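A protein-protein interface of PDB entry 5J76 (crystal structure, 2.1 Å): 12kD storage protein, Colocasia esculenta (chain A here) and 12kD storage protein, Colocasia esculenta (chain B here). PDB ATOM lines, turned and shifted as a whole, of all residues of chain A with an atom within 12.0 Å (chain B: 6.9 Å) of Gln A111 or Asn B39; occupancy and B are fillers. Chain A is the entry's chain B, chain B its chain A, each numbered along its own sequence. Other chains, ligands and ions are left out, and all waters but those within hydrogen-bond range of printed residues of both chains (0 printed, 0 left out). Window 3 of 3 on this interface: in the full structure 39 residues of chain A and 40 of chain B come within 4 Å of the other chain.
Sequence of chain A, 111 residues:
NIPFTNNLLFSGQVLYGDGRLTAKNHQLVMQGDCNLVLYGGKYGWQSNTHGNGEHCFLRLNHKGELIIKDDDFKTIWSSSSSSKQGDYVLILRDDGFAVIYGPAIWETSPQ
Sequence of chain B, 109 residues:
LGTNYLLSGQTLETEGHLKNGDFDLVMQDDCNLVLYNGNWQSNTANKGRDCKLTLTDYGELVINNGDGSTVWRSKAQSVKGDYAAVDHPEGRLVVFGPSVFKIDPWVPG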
ATOM      1  N   TRP A 106      27.397 -14.914  29.754  1.00  0.00           N
ATOM      2  CA  TRP A 106      26.545 -15.435  28.722  1.00  0.00           C
ATOM      3  C   TRP A 106      25.628 -16.443  29.372  1.00  0.00           C
ATOM      4  O   TRP A 106      26.039 -17.116  30.299  1.00  0.00           O
ATOM      5  CB  TRP A 106      27.395 -16.150  27.697  1.00  0.00           C
ATOM      6  CG  TRP A 106      26.599 -16.679  26.548  1.00  0.00           C
ATOM      7  CD1 TRP A 106      26.307 -16.021  25.386  1.00  0.00           C
ATOM      8  CD2 TRP A 106      26.007 -17.971  26.441  1.00  0.00           C
ATOM      9  NE1 TRP A 106      25.577 -16.832  24.567  1.00  0.00           N
ATOM     10  CE2 TRP A 106      25.369 -18.030  25.192  1.00  0.00           C
ATOM     11  CE3 TRP A 106      25.950 -19.086  27.288  1.00  0.00           C
ATOM     12  CZ2 TRP A 106      24.710 -19.157  24.752  1.00  0.00           C
ATOM     13  CZ3 TRP A 106      25.288 -20.190  26.862  1.00  0.00           C
ATOM     14  CH2 TRP A 106      24.684 -20.243  25.586  1.00  0.00           C
ATOM     15  N   GLU A 107      24.399 -16.534  28.912  1.00  0.00           N
ATOM     16  CA  GLU A 107      23.501 -17.591  29.400  1.00  0.00           C
ATOM     17  C   GLU A 107      22.526 -17.969  28.350  1.00  0.00           C
ATOM     18  O   GLU A 107      22.262 -17.176  27.454  1.00  0.00           O
ATOM     19  CB  GLU A 107      22.775 -17.145  30.644  1.00  0.00           C
ATOM     20  CG  GLU A 107      21.709 -16.078  30.438  1.00  0.00           C
ATOM     21  CD  GLU A 107      21.222 -15.524  31.793  1.00  0.00           C
ATOM     22  OE1 GLU A 107      21.033 -14.317  31.861  1.00  0.00           O
ATOM     23  OE2 GLU A 107      21.070 -16.273  32.801  1.00  0.00           O
ATOM     24  N   THR A 108      22.019 -19.195  28.407  1.00  0.00           N
ATOM     25  CA  THR A 108      20.918 -19.601  27.514  1.00  0.00           C
ATOM     26  C   THR A 108      19.652 -18.887  27.932  1.00  0.00           C
ATOM     27  O   THR A 108      19.437 -18.599  29.106  1.00  0.00           O
ATOM     28  CB  THR A 108      20.622 -21.103  27.604  1.00  0.00           C
ATOM     29  OG1 THR A 108      20.375 -21.415  28.975  1.00  0.00           O
ATOM     30  CG2 THR A 108      21.833 -21.945  27.033  1.00  0.00           C
ATOM     31  N   SER A 109      18.801 -18.604  26.973  1.00  0.00           N
ATOM     32  CA  SER A 109      17.456 -18.109  27.330  1.00  0.00           C
ATOM     33  C   SER A 109      16.311 -18.875  26.562  1.00  0.00           C
ATOM     34  O   SER A 109      16.437 -19.120  25.348  1.00  0.00           O
ATOM     35  CB  SER A 109      17.427 -16.574  27.132  1.00  0.00           C
ATOM     36  OG  SER A 109      17.823 -15.934  28.341  1.00  0.00           O
ATOM     37  N   PRO A 110      15.207 -19.258  27.263  1.00  0.00           N
ATOM     38  CA  PRO A 110      14.024 -19.858  26.575  1.00  0.00           C
ATOM     39  C   PRO A 110      13.647 -19.210  25.213  1.00  0.00           C
ATOM     40  O   PRO A 110      13.581 -17.990  25.140  1.00  0.00           O
ATOM     41  CB  PRO A 110      12.911 -19.705  27.629  1.00  0.00           C
ATOM     42  CG  PRO A 110      13.649 -19.930  28.925  1.00  0.00           C
ATOM     43  CD  PRO A 110      15.024 -19.279  28.736  1.00  0.00           C
ATOM     44  N   GLN A 111      13.420 -20.027  24.169  1.00  0.00           N
ATOM     45  CA  GLN A 111      13.414 -19.581  22.740  1.00  0.00           C
ATOM     46  C   GLN A 111      12.011 -19.497  22.093  1.00  0.00           C
ATOM     47  O   GLN A 111      11.106 -20.264  22.423  1.00  0.00           O
ATOM     48  CB  GLN A 111      14.350 -20.492  21.888  1.00  0.00           C
ATOM     49  CG  GLN A 111      15.850 -20.110  21.937  1.00  0.00           C
ATOM     50  CD  GLN A 111      16.835 -21.211  21.441  1.00  0.00           C
ATOM     51  OE1 GLN A 111      16.492 -22.390  21.367  1.00  0.00           O
ATOM     52  NE2 GLN A 111      18.079 -20.818  21.126  1.00  0.00           N
ATOM     53  N   PHE B  23      17.028 -30.695  34.543  1.00  0.00           N
ATOM     54  CA  PHE B  23      17.610 -30.132  33.367  1.00  0.00           C
ATOM     55  C   PHE B  23      18.758 -30.992  32.916  1.00  0.00           C
ATOM     56  O   PHE B  23      19.535 -31.474  33.724  1.00  0.00           O
ATOM     57  CB  PHE B  23      17.961 -28.674  33.605  1.00  0.00           C
ATOM     58  CG  PHE B  23      16.785 -27.872  34.091  1.00  0.00           C
ATOM     59  CD1 PHE B  23      15.775 -27.485  33.206  1.00  0.00           C
ATOM     60  CD2 PHE B  23      16.640 -27.564  35.449  1.00  0.00           C
ATOM     61  CE1 PHE B  23      14.676 -26.768  33.671  1.00  0.00           C
ATOM     62  CE2 PHE B  23      15.551 -26.837  35.912  1.00  0.00           C
ATOM     63  CZ  PHE B  23      14.569 -26.422  35.031  1.00  0.00           C
ATOM     64  N   LEU B  35      19.214 -28.394  25.702  1.00  0.00           N
ATOM     65  CA  LEU B  35      19.030 -28.294  27.113  1.00  0.00           C
ATOM     66  C   LEU B  35      17.610 -28.723  27.379  1.00  0.00           C
ATOM     67  O   LEU B  35      16.650 -27.883  27.304  1.00  0.00           O
ATOM     68  CB  LEU B  35      19.290 -26.883  27.579  1.00  0.00           C
ATOM     69  CG  LEU B  35      19.046 -26.533  29.083  1.00  0.00           C
ATOM     70  CD1 LEU B  35      19.476 -27.593  30.012  1.00  0.00           C
ATOM     71  CD2 LEU B  35      19.727 -25.242  29.480  1.00  0.00           C
ATOM     72  N   TYR B  36      17.458 -30.016  27.675  1.00  0.00           N
ATOM     73  CA  TYR B  36      16.113 -30.590  27.986  1.00  0.00           C
ATOM     74  C   TYR B  36      15.489 -29.924  29.196  1.00  0.00           C
ATOM     75  O   TYR B  36      16.143 -29.720  30.231  1.00  0.00           O
ATOM     76  CB  TYR B  36      16.106 -32.099  28.122  1.00  0.00           C
ATOM     77  CG  TYR B  36      16.299 -32.749  26.749  1.00  0.00           C
ATOM     78  CD1 TYR B  36      15.201 -32.934  25.883  1.00  0.00           C
ATOM     79  CD2 TYR B  36      17.579 -33.067  26.268  1.00  0.00           C
ATOM     80  CE1 TYR B  36      15.394 -33.435  24.595  1.00  0.00           C
ATOM     81  CE2 TYR B  36      17.768 -33.593  24.981  1.00  0.00           C
ATOM     82  CZ  TYR B  36      16.664 -33.766  24.150  1.00  0.00           C
ATOM     83  OH  TYR B  36      16.805 -34.280  22.881  1.00  0.00           O
ATOM     84  N   ASN B  37      14.236 -29.563  29.005  1.00  0.00           N
ATOM     85  CA  ASN B  37      13.385 -28.794  29.929  1.00  0.00           C
ATOM     86  C   ASN B  37      13.777 -27.366  30.061  1.00  0.00           C
ATOM     87  O   ASN B  37      13.120 -26.657  30.795  1.00  0.00           O
ATOM     88  CB  ASN B  37      13.262 -29.477  31.302  1.00  0.00           C
ATOM     89  CG  ASN B  37      12.442 -30.712  31.213  1.00  0.00           C
ATOM     90  OD1 ASN B  37      11.469 -30.697  30.525  1.00  0.00           O
ATOM     91  ND2 ASN B  37      12.856 -31.794  31.829  1.00  0.00           N
ATOM     92  N   GLY B  38      14.847 -26.933  29.373  1.00  0.00           N
ATOM     93  CA  GLY B  38      15.217 -25.554  29.392  1.00  0.00           C
ATOM     94  C   GLY B  38      14.820 -24.748  28.195  1.00  0.00           C
ATOM     95  O   GLY B  38      15.242 -23.601  28.116  1.00  0.00           O
ATOM     96  N   ASN B  39      14.083 -25.324  27.256  1.00  0.00           N
ATOM     97  CA  ASN B  39      13.682 -24.600  25.999  1.00  0.00           C
ATOM     98  C   ASN B  39      14.813 -23.932  25.304  1.00  0.00           C
ATOM     99  O   ASN B  39      14.767 -22.733  25.004  1.00  0.00           O
ATOM    100  CB  ASN B  39      12.638 -23.524  26.297  1.00  0.00           C
ATOM    101  CG  ASN B  39      11.460 -24.091  27.025  1.00  0.00           C
ATOM    102  OD1 ASN B  39      11.465 -24.217  28.262  1.00  0.00           O
ATOM    103  ND2 ASN B  39      10.454 -24.478  26.265  1.00  0.00           N
ATOM    104  N   TRP B  40      15.887 -24.660  25.089  1.00  0.00           N
ATOM    105  CA  TRP B  40      16.996 -24.049  24.400  1.00  0.00           C
ATOM    106  C   TRP B  40      17.731 -25.131  23.651  1.00  0.00           C
ATOM    107  O   TRP B  40      17.910 -26.268  24.156  1.00  0.00           O
ATOM    108  CB  TRP B  40      17.947 -23.414  25.410  1.00  0.00           C
ATOM    109  CG  TRP B  40      19.069 -22.679  24.736  1.00  0.00           C
ATOM    110  CD1 TRP B  40      19.072 -21.347  24.399  1.00  0.00           C
ATOM    111  CD2 TRP B  40      20.346 -23.196  24.295  1.00  0.00           C
ATOM    112  NE1 TRP B  40      20.250 -21.014  23.759  1.00  0.00           N
ATOM    113  CE2 TRP B  40      21.059 -22.100  23.693  1.00  0.00           C
ATOM    114  CE3 TRP B  40      20.950 -24.449  24.322  1.00  0.00           C
ATOM    115  CZ2 TRP B  40      22.339 -22.238  23.145  1.00  0.00           C
ATOM    116  CZ3 TRP B  40      22.221 -24.606  23.757  1.00  0.00           C
ATOM    117  CH2 TRP B  40      22.907 -23.506  23.191  1.00  0.00           C
ATOM    118  N   GLN B  41      18.253 -24.747  22.503  1.00  0.00           N
ATOM    119  CA  GLN B  41      19.125 -25.602  21.736  1.00  0.00           C
ATOM    120  C   GLN B  41      20.063 -24.732  20.905  1.00  0.00           C
ATOM    121  O   GLN B  41      19.740 -23.622  20.560  1.00  0.00           O
ATOM    122  CB  GLN B  41      18.272 -26.480  20.821  1.00  0.00           C
ATOM    123  CG  GLN B  41      17.302 -25.687  19.908  1.00  0.00           C
ATOM    124  CD  GLN B  41      16.554 -26.633  18.979  1.00  0.00           C
ATOM    125  OE1 GLN B  41      15.526 -27.176  19.314  1.00  0.00           O
ATOM    126  NE2 GLN B  41      17.143 -26.928  17.903  1.00  0.00           N
ATOM    127  N   SER B  42      21.206 -25.283  20.537  1.00  0.00           N
ATOM    128  CA  SER B  42      22.087 -24.593  19.661  1.00  0.00           C
ATOM    129  C   SER B  42      21.523 -24.489  18.237  1.00  0.00           C
ATOM    130  O   SER B  42      22.036 -23.727  17.412  1.00  0.00           O
ATOM    131  CB  SER B  42      23.432 -25.281  19.560  1.00  0.00           C
ATOM    132  OG  SER B  42      23.266 -26.597  19.085  1.00  0.00           O
ATOM    133  N   ASN B  43      20.534 -25.310  17.951  1.00  0.00           N
ATOM    134  CA  ASN B  43      19.957 -25.413  16.642  1.00  0.00           C
ATOM    135  C   ASN B  43      20.978 -25.805  15.563  1.00  0.00           C
ATOM    136  O   ASN B  43      21.101 -25.159  14.552  1.00  0.00           O
ATOM    137  CB  ASN B  43      19.205 -24.103  16.352  1.00  0.00           C
ATOM    138  CG  ASN B  43      18.255 -24.239  15.207  1.00  0.00           C
ATOM    139  OD1 ASN B  43      17.685 -25.310  14.953  1.00  0.00           O
ATOM    140  ND2 ASN B  43      18.096 -23.157  14.473  1.00  0.00           N
ATOM    141  N   GLY B  91      17.553 -24.047  35.303  1.00  0.00           N
ATOM    142  CA  GLY B  91      17.346 -24.432  33.945  1.00  0.00           C
ATOM    143  C   GLY B  91      18.014 -23.570  32.882  1.00  0.00           C
ATOM    144  O   GLY B  91      17.540 -23.496  31.784  1.00  0.00           O
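The backbone NH (N) of Gln A111 lies within hydrogen-bond range of the backbone carbonyl oxygen (O) of Asn B39, 3.1 Å away. NE1 of Trp B40 sits close to NE2 of Gln A111 (3.4 Å). N of Gln B41 lies within hydrogen-bond range of OE1 of Gln A111 (3.2 Å).
The backbone carbonyl oxygen of Trp B40 sits at hydrogen-bond distance from the backbone NH of Leu B35. NE2 of Gln B41 lies within hydrogen-bond range of OD1 of Asn B43.
Among the printed residues, merely in contact across the chains: Thr A108 with Trp B40 (3.4 Å), Pro A110 with Asn B39 (3.4 Å), Ser A109 with Trp B40 (3.6 Å), Thr A108 with Leu B35 (3.9 Å), Trp A106 with Trp B40 (3.9 Å) and Ser A109 with Asn B39 (3.995 Å).
Of the printed residues of chain B, Trp A106 touches Trp B40. Of the printed residues of chain B, Thr A108 touches Leu B35 and Trp B40. Of the printed residues of chain B, Ser A109 touches Asn B39 (3.995 Å) and Trp B40 (3.6 Å). Printed residues of chain B within 4 Å of Pro A110: Asn B39. Gln A111 touches just these residues of chain B: Asn B39 (3.1 Å), Trp B40 (3.4 Å) and Gln B41 (3.2 Å). Of chain A, only Thr A108 comes within 4 Å of Leu B35. Of the printed residues of chain A, Trp B40 touches Trp A106 (3.9 Å), Thr A108 (3.4 Å), Ser A109 (3.6 Å) and Gln A111 (3.4 Å). Gln B41 touches just one residue of chain A: Gln A111. The nearest printed residue of chain A that does not touch Asn B39 is Thr A108 (6.6 Å). The nearest printed residue of chain B that does not touch Thr A108 is Gly B91 (4.5 Å).
Hydrophobic or aromatic side chains of chain B within 4 Å of the printed part of chain A: Leu B35 and Trp B40. Of the 6 printed residues of chain A, 5 touch a printed residue of chain B. Hydrophobic or aromatic side chains of chain A within 4 Å of the printed part of chain B: Trp A106. Along chain A the printed residues that touch a printed residue of chain B span positions 106 to 111. Among the printed residues, no Asp or Glu carboxylate lies within 4 Å of a Lys or Arg side-chain nitrogen of the other chain.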
